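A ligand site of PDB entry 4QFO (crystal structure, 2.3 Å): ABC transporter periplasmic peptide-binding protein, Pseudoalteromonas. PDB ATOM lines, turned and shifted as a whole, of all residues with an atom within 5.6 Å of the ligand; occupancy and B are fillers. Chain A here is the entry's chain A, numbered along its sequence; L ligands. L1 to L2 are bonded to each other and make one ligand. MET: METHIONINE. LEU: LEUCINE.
The backbone NH (N) of Gly 50 lies within hydrogen-bond range of an oxygen (O) of LEU L2 (2.8 Å).
A nitrogen (N) of LEU L2 sits at hydrogen-bond distance from the backbone carbonyl oxygen (O) of Thr 48, at 2.8 Å.
An oxygen (O) of MET L1 lies within hydrogen-bond range of the backbone NH (N) of Ala 434 (2.9 Å).
The side-chain carboxylate (OD1) of Asp 436 is in salt-bridge range of a nitrogen (N) of MET L1 (2.8 Å).
The backbone carbonyl oxygen (O) of Ala 434 is in hydrogen-bond range of a nitrogen (N) of MET L1 (2.9 Å).
OH of Tyr 385 is in hydrogen-bond range of OXT of LEU L2 (2.6 Å).
OXT of LEU L2 is in salt-bridge range of NE of Arg 383 (3.0 Å).
Residues that only touch the ligand: Trp 433, Ile 418, Ile 53, Trp 414, Ala 526, Phe 182, Gly 432 and Thr 49.
Within 4 Å of the ligand: Thr 48, Thr 49, Gly 50, Ile 53, Phe 182, Arg 383, Tyr 385, Trp 414, Ile 418, Gly 432, Trp 433, Ala 434, Asp 436 and Ala 526.
The nearest printed residue that does not touch the ligand is Asp 181 (4.01 Å).
OD2 of Asp 181 lies within hydrogen-bond range of N of Ala 526 (2.8 Å).
NE1 of Trp 414 lies within hydrogen-bond range of OG of Ser 51 (2.9 Å).
NE1 of Trp 433 sits close to ND2 of Asn 442 (2.8 Å).
ND2 of Asn 442 lies close to N of Asp 436.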
ATOM      1  N   THR A  48      -8.561  26.481  19.782  1.00  0.00           N
ATOM      2  CA  THR A  48      -9.798  26.063  20.439  1.00  0.00           C
ATOM      3  C   THR A  48     -10.920  27.034  20.131  1.00  0.00           C
ATOM      4  O   THR A  48     -11.989  26.963  20.726  1.00  0.00           O
ATOM      5  CB  THR A  48      -9.649  25.931  21.983  1.00  0.00           C
ATOM      6  OG1 THR A  48      -9.180  27.169  22.546  1.00  0.00           O
ATOM      7  CG2 THR A  48      -8.677  24.796  22.321  1.00  0.00           C
ATOM      8  N   THR A  49     -10.691  27.920  19.169  1.00  0.00           N
ATOM      9  CA  THR A  49     -11.649  28.976  18.851  1.00  0.00           C
ATOM     10  C   THR A  49     -12.729  28.485  17.903  1.00  0.00           C
ATOM     11  O   THR A  49     -12.432  28.093  16.769  1.00  0.00           O
ATOM     12  CB  THR A  49     -10.911  30.196  18.238  1.00  0.00           C
ATOM     13  OG1 THR A  49     -10.000  30.719  19.202  1.00  0.00           O
ATOM     14  CG2 THR A  49     -11.887  31.295  17.803  1.00  0.00           C
ATOM     15  N   GLY A  50     -13.981  28.527  18.367  1.00  0.00           N
ATOM     16  CA  GLY A  50     -15.087  27.945  17.629  1.00  0.00           C
ATOM     17  C   GLY A  50     -15.363  28.583  16.283  1.00  0.00           C
ATOM     18  O   GLY A  50     -15.873  27.922  15.359  1.00  0.00           O
ATOM     19  N   SER A  51     -15.033  29.862  16.146  1.00  0.00           N
ATOM     20  CA  SER A  51     -15.257  30.578  14.897  1.00  0.00           C
ATOM     21  C   SER A  51     -14.414  29.953  13.817  1.00  0.00           C
ATOM     22  O   SER A  51     -14.835  29.865  12.658  1.00  0.00           O
ATOM     23  CB  SER A  51     -14.905  32.061  15.043  1.00  0.00           C
ATOM     24  OG  SER A  51     -15.552  32.601  16.169  1.00  0.00           O
ATOM     25  N   ILE A  53     -13.103  26.658  14.004  1.00  0.00           N
ATOM     26  CA  ILE A  53     -13.552  25.274  13.896  1.00  0.00           C
ATOM     27  C   ILE A  53     -14.823  25.149  13.048  1.00  0.00           C
ATOM     28  O   ILE A  53     -14.971  24.216  12.252  1.00  0.00           O
ATOM     29  CB  ILE A  53     -13.838  24.681  15.285  1.00  0.00           C
ATOM     30  CG1 ILE A  53     -12.630  24.895  16.184  1.00  0.00           C
ATOM     31  CG2 ILE A  53     -14.159  23.200  15.166  1.00  0.00           C
ATOM     32  CD1 ILE A  53     -11.336  24.384  15.542  1.00  0.00           C
ATOM     33  N   ASP A  54     -15.736  26.095  13.243  1.00  0.00           N
ATOM     34  CA  ASP A  54     -16.988  26.086  12.510  1.00  0.00           C
ATOM     35  C   ASP A  54     -16.754  26.166  11.009  1.00  0.00           C
ATOM     36  O   ASP A  54     -17.495  25.569  10.240  1.00  0.00           O
ATOM     37  CB  ASP A  54     -17.877  27.239  12.978  1.00  0.00           C
ATOM     38  CG  ASP A  54     -18.725  26.866  14.158  1.00  0.00           C
ATOM     39  OD1 ASP A  54     -18.762  25.658  14.493  1.00  0.00           O
ATOM     40  OD2 ASP A  54     -19.372  27.761  14.741  1.00  0.00           O
ATOM     41  N   ASP A 181     -13.714  17.897  17.316  1.00  0.00           N
ATOM     42  CA  ASP A 181     -13.431  18.503  16.026  1.00  0.00           C
ATOM     43  C   ASP A 181     -11.940  18.808  15.884  1.00  0.00           C
ATOM     44  O   ASP A 181     -11.476  19.136  14.777  1.00  0.00           O
ATOM     45  CB  ASP A 181     -14.231  19.804  15.856  1.00  0.00           C
ATOM     46  CG  ASP A 181     -15.731  19.591  15.942  1.00  0.00           C
ATOM     47  OD1 ASP A 181     -16.265  18.774  15.155  1.00  0.00           O
ATOM     48  OD2 ASP A 181     -16.379  20.228  16.802  1.00  0.00           O
ATOM     49  N   PHE A 182     -11.207  18.712  16.990  1.00  0.00           N
ATOM     50  CA  PHE A 182      -9.764  18.989  16.968  1.00  0.00           C
ATOM     51  C   PHE A 182      -8.998  17.793  16.434  1.00  0.00           C
ATOM     52  O   PHE A 182      -7.894  17.943  15.903  1.00  0.00           O
ATOM     53  CB  PHE A 182      -9.267  19.398  18.361  1.00  0.00           C
ATOM     54  CG  PHE A 182     -10.112  20.453  19.018  1.00  0.00           C
ATOM     55  CD1 PHE A 182     -10.171  21.728  18.509  1.00  0.00           C
ATOM     56  CD2 PHE A 182     -10.868  20.151  20.140  1.00  0.00           C
ATOM     57  CE1 PHE A 182     -10.968  22.692  19.112  1.00  0.00           C
ATOM     58  CE2 PHE A 182     -11.667  21.125  20.756  1.00  0.00           C
ATOM     59  CZ  PHE A 182     -11.709  22.391  20.237  1.00  0.00           C
ATOM     60  N   ARG A 383     -21.581  34.646  21.337  1.00  0.00           N
ATOM     61  CA  ARG A 383     -21.299  33.205  21.465  1.00  0.00           C
ATOM     62  C   ARG A 383     -22.543  32.483  22.022  1.00  0.00           C
ATOM     63  O   ARG A 383     -23.459  33.102  22.525  1.00  0.00           O
ATOM     64  CB  ARG A 383     -20.095  32.899  22.386  1.00  0.00           C
ATOM     65  CG  ARG A 383     -18.919  33.876  22.327  1.00  0.00           C
ATOM     66  CD  ARG A 383     -18.276  33.955  20.955  1.00  0.00           C
ATOM     67  NE  ARG A 383     -17.743  32.676  20.495  1.00  0.00           N
ATOM     68  CZ  ARG A 383     -17.973  32.169  19.283  1.00  0.00           C
ATOM     69  NH1 ARG A 383     -18.740  32.829  18.408  1.00  0.00           N
ATOM     70  NH2 ARG A 383     -17.434  31.005  18.935  1.00  0.00           N
ATOM     71  N   TYR A 385     -22.740  30.771  24.623  1.00  0.00           N
ATOM     72  CA  TYR A 385     -22.794  30.942  26.064  1.00  0.00           C
ATOM     73  C   TYR A 385     -23.062  32.369  26.487  1.00  0.00           C
ATOM     74  O   TYR A 385     -23.366  32.625  27.650  1.00  0.00           O
ATOM     75  CB  TYR A 385     -21.514  30.403  26.729  1.00  0.00           C
ATOM     76  CG  TYR A 385     -20.216  30.802  26.055  1.00  0.00           C
ATOM     77  CD1 TYR A 385     -19.612  32.018  26.345  1.00  0.00           C
ATOM     78  CD2 TYR A 385     -19.587  29.946  25.152  1.00  0.00           C
ATOM     79  CE1 TYR A 385     -18.413  32.381  25.760  1.00  0.00           C
ATOM     80  CE2 TYR A 385     -18.393  30.304  24.554  1.00  0.00           C
ATOM     81  CZ  TYR A 385     -17.813  31.523  24.852  1.00  0.00           C
ATOM     82  OH  TYR A 385     -16.621  31.892  24.268  1.00  0.00           O
ATOM     83  N   TRP A 414     -12.020  39.629  17.957  1.00  0.00           N
ATOM     84  CA  TRP A 414     -12.180  38.313  18.577  1.00  0.00           C
ATOM     85  C   TRP A 414     -10.891  37.513  18.744  1.00  0.00           C
ATOM     86  O   TRP A 414     -10.536  37.140  19.859  1.00  0.00           O
ATOM     87  CB  TRP A 414     -13.218  37.508  17.788  1.00  0.00           C
ATOM     88  CG  TRP A 414     -13.636  36.147  18.331  1.00  0.00           C
ATOM     89  CD1 TRP A 414     -13.957  35.049  17.582  1.00  0.00           C
ATOM     90  CD2 TRP A 414     -13.821  35.768  19.710  1.00  0.00           C
ATOM     91  NE1 TRP A 414     -14.320  34.009  18.398  1.00  0.00           N
ATOM     92  CE2 TRP A 414     -14.253  34.421  19.702  1.00  0.00           C
ATOM     93  CE3 TRP A 414     -13.655  36.417  20.926  1.00  0.00           C
ATOM     94  CZ2 TRP A 414     -14.512  33.718  20.879  1.00  0.00           C
ATOM     95  CZ3 TRP A 414     -13.927  35.716  22.091  1.00  0.00           C
ATOM     96  CH2 TRP A 414     -14.354  34.378  22.055  1.00  0.00           C
ATOM     97  N   ILE A 418      -8.816  36.883  22.239  1.00  0.00           N
ATOM     98  CA  ILE A 418      -8.426  35.591  22.784  1.00  0.00           C
ATOM     99  C   ILE A 418      -6.922  35.507  23.080  1.00  0.00           C
ATOM    100  O   ILE A 418      -6.489  35.048  24.138  1.00  0.00           O
ATOM    101  CB  ILE A 418      -8.870  34.468  21.837  1.00  0.00           C
ATOM    102  CG1 ILE A 418     -10.383  34.265  21.956  1.00  0.00           C
ATOM    103  CG2 ILE A 418      -8.103  33.192  22.107  1.00  0.00           C
ATOM    104  CD1 ILE A 418     -10.955  33.314  20.918  1.00  0.00           C
ATOM    105  N   LEU A 431     -15.919  35.324  29.465  1.00  0.00           N
ATOM    106  CA  LEU A 431     -15.663  34.287  28.477  1.00  0.00           C
ATOM    107  C   LEU A 431     -16.584  33.094  28.686  1.00  0.00           C
ATOM    108  O   LEU A 431     -17.619  33.210  29.336  1.00  0.00           O
ATOM    109  CB  LEU A 431     -14.201  33.850  28.513  1.00  0.00           C
ATOM    110  CG  LEU A 431     -13.358  34.207  27.284  1.00  0.00           C
ATOM    111  CD1 LEU A 431     -11.950  33.661  27.414  1.00  0.00           C
ATOM    112  CD2 LEU A 431     -14.016  33.700  26.015  1.00  0.00           C
ATOM    113  N   GLY A 432     -16.204  31.940  28.136  1.00  0.00           N
ATOM    114  CA  GLY A 432     -17.016  30.748  28.257  1.00  0.00           C
ATOM    115  C   GLY A 432     -16.509  29.560  27.472  1.00  0.00           C
ATOM    116  O   GLY A 432     -15.379  29.547  26.998  1.00  0.00           O
ATOM    117  N   TRP A 433     -17.364  28.554  27.338  1.00  0.00           N
ATOM    118  CA  TRP A 433     -17.010  27.325  26.664  1.00  0.00           C
ATOM    119  C   TRP A 433     -18.273  26.691  26.097  1.00  0.00           C
ATOM    120  O   TRP A 433     -19.257  26.534  26.804  1.00  0.00           O
ATOM    121  CB  TRP A 433     -16.322  26.386  27.647  1.00  0.00           C
ATOM    122  CG  TRP A 433     -15.704  25.129  27.070  1.00  0.00           C
ATOM    123  CD1 TRP A 433     -16.200  23.864  27.163  1.00  0.00           C
ATOM    124  CD2 TRP A 433     -14.487  25.023  26.324  1.00  0.00           C
ATOM    125  NE1 TRP A 433     -15.366  22.977  26.538  1.00  0.00           N
ATOM    126  CE2 TRP A 433     -14.306  23.664  26.016  1.00  0.00           C
ATOM    127  CE3 TRP A 433     -13.531  25.949  25.884  1.00  0.00           C
ATOM    128  CZ2 TRP A 433     -13.213  23.193  25.280  1.00  0.00           C
ATOM    129  CZ3 TRP A 433     -12.429  25.483  25.183  1.00  0.00           C
ATOM    130  CH2 TRP A 433     -12.284  24.113  24.877  1.00  0.00           C
ATOM    131  N   ALA A 434     -18.253  26.396  24.802  1.00  0.00           N
ATOM    132  CA  ALA A 434     -19.274  25.541  24.181  1.00  0.00           C
ATOM    133  C   ALA A 434     -18.632  24.172  24.070  1.00  0.00           C
ATOM    134  O   ALA A 434     -17.637  24.012  23.378  1.00  0.00           O
ATOM    135  CB  ALA A 434     -19.651  26.045  22.828  1.00  0.00           C
ATOM    136  N   ALA A 435     -19.178  23.207  24.807  1.00  0.00           N
ATOM    137  CA  ALA A 435     -18.545  21.915  24.944  1.00  0.00           C
ATOM    138  C   ALA A 435     -18.328  21.226  23.594  1.00  0.00           C
ATOM    139  O   ALA A 435     -19.124  21.393  22.671  1.00  0.00           O
ATOM    140  CB  ALA A 435     -19.368  21.031  25.887  1.00  0.00           C
ATOM    141  N   ASP A 436     -17.232  20.467  23.499  1.00  0.00           N
ATOM    142  CA  ASP A 436     -16.865  19.730  22.296  1.00  0.00           C
ATOM    143  C   ASP A 436     -17.461  18.328  22.297  1.00  0.00           C
ATOM    144  O   ASP A 436     -17.680  17.733  21.250  1.00  0.00           O
ATOM    145  CB  ASP A 436     -15.337  19.654  22.194  1.00  0.00           C
ATOM    146  CG  ASP A 436     -14.654  20.999  22.454  1.00  0.00           C
ATOM    147  OD1 ASP A 436     -14.752  21.903  21.595  1.00  0.00           O
ATOM    148  OD2 ASP A 436     -14.033  21.131  23.531  1.00  0.00           O
ATOM    149  N   ASN A 442     -14.687  17.698  29.616  1.00  0.00           N
ATOM    150  CA  ASN A 442     -14.546  18.763  28.624  1.00  0.00           C
ATOM    151  C   ASN A 442     -14.788  20.169  29.193  1.00  0.00           C
ATOM    152  O   ASN A 442     -14.408  21.153  28.585  1.00  0.00           O
ATOM    153  CB  ASN A 442     -15.487  18.485  27.438  1.00  0.00           C
ATOM    154  CG  ASN A 442     -15.144  19.309  26.208  1.00  0.00           C
ATOM    155  OD1 ASN A 442     -14.159  19.030  25.517  1.00  0.00           O
ATOM    156  ND2 ASN A 442     -15.965  20.307  25.903  1.00  0.00           N
ATOM    157  N   LYS A 457      -5.015  29.115  28.053  1.00  0.00           N
ATOM    158  CA  LYS A 457      -6.458  29.013  27.823  1.00  0.00           C
ATOM    159  C   LYS A 457      -7.272  28.945  29.108  1.00  0.00           C
ATOM    160  O   LYS A 457      -8.472  28.649  29.098  1.00  0.00           O
ATOM    161  CB  LYS A 457      -6.780  27.793  26.938  1.00  0.00           C
ATOM    162  CG  LYS A 457      -6.130  27.848  25.570  1.00  0.00           C
ATOM    163  CD  LYS A 457      -6.598  29.030  24.711  1.00  0.00           C
ATOM    164  CE  LYS A 457      -5.761  29.079  23.424  1.00  0.00           C
ATOM    165  NZ  LYS A 457      -6.105  30.202  22.480  1.00  0.00           N
ATOM    166  N   ARG A 508     -28.523  27.392  21.605  1.00  0.00           N
ATOM    167  CA  ARG A 508     -27.792  27.509  20.376  1.00  0.00           C
ATOM    168  C   ARG A 508     -28.721  27.978  19.276  1.00  0.00           C
ATOM    169  O   ARG A 508     -29.595  27.228  18.818  1.00  0.00           O
ATOM    170  CB  ARG A 508     -27.133  26.175  20.035  1.00  0.00           C
ATOM    171  CG  ARG A 508     -26.147  26.240  18.883  1.00  0.00           C
ATOM    172  CD  ARG A 508     -25.485  24.889  18.696  1.00  0.00           C
ATOM    173  NE  ARG A 508     -24.246  25.013  17.934  1.00  0.00           N
ATOM    174  CZ  ARG A 508     -23.377  24.029  17.751  1.00  0.00           C
ATOM    175  NH1 ARG A 508     -23.621  22.816  18.253  1.00  0.00           N
ATOM    176  NH2 ARG A 508     -22.274  24.247  17.050  1.00  0.00           N
ATOM    177  N   GLY A 525     -20.213  20.321  20.118  1.00  0.00           N
ATOM    178  CA  GLY A 525     -19.459  20.281  18.873  1.00  0.00           C
ATOM    179  C   GLY A 525     -19.734  21.385  17.871  1.00  0.00           C
ATOM    180  O   GLY A 525     -20.683  22.143  17.988  1.00  0.00           O
ATOM    181  N   ALA A 526     -18.887  21.453  16.857  1.00  0.00           N
ATOM    182  CA  ALA A 526     -18.947  22.515  15.864  1.00  0.00           C
ATOM    183  C   ALA A 526     -20.052  22.303  14.822  1.00  0.00           C
ATOM    184  O   ALA A 526     -20.508  21.188  14.610  1.00  0.00           O
ATOM    185  CB  ALA A 526     -17.582  22.639  15.164  1.00  0.00           C
ATOM    186  N   ILE A 527     -20.460  23.385  14.184  1.00  0.00           N
ATOM    187  CA  ILE A 527     -21.395  23.353  13.069  1.00  0.00           C
ATOM    188  C   ILE A 527     -20.888  22.425  11.974  1.00  0.00           C
ATOM    189  O   ILE A 527     -19.685  22.359  11.718  1.00  0.00           O
ATOM    190  CB  ILE A 527     -21.548  24.748  12.457  1.00  0.00           C
ATOM    191  CG1 ILE A 527     -22.244  25.669  13.444  1.00  0.00           C
ATOM    192  CG2 ILE A 527     -22.318  24.689  11.145  1.00  0.00           C
ATOM    193  CD1 ILE A 527     -23.381  24.995  14.119  1.00  0.00           C
HETATM  194  N   MET L   1     -14.774  24.455  22.827  1.00  0.00           N
HETATM  195  CA  MET L   1     -14.598  25.567  21.910  1.00  0.00           C
HETATM  196  C   MET L   1     -14.920  26.916  22.543  1.00  0.00           C
HETATM  197  O   MET L   1     -15.898  27.060  23.265  1.00  0.00           O
HETATM  198  CB  MET L   1     -15.483  25.393  20.670  1.00  0.00           C
HETATM  199  CG  MET L   1     -14.841  24.528  19.607  1.00  0.00           C
HETATM  200  SD  MET L   1     -16.003  23.904  18.368  1.00  0.00           S
HETATM  201  CE  MET L   1     -17.298  25.148  18.420  1.00  0.00           C
HETATM  202  N   LEU L   2     -14.091  27.906  22.242  1.00  0.00           N
HETATM  203  CA  LEU L   2     -14.372  29.275  22.633  1.00  0.00           C
HETATM  204  C   LEU L   2     -15.445  29.802  21.688  1.00  0.00           C
HETATM  205  O   LEU L   2     -15.457  29.423  20.510  1.00  0.00           O
HETATM  206  CB  LEU L   2     -13.110  30.118  22.481  1.00  0.00           C
HETATM  207  CG  LEU L   2     -12.185  30.376  23.679  1.00  0.00           C
HETATM  208  CD1 LEU L   2     -12.257  29.264  24.699  1.00  0.00           C
HETATM  209  CD2 LEU L   2     -10.757  30.620  23.209  1.00  0.00           C
HETATM  210  OXT LEU L   2     -16.311  30.608  22.058  1.00  0.00           O
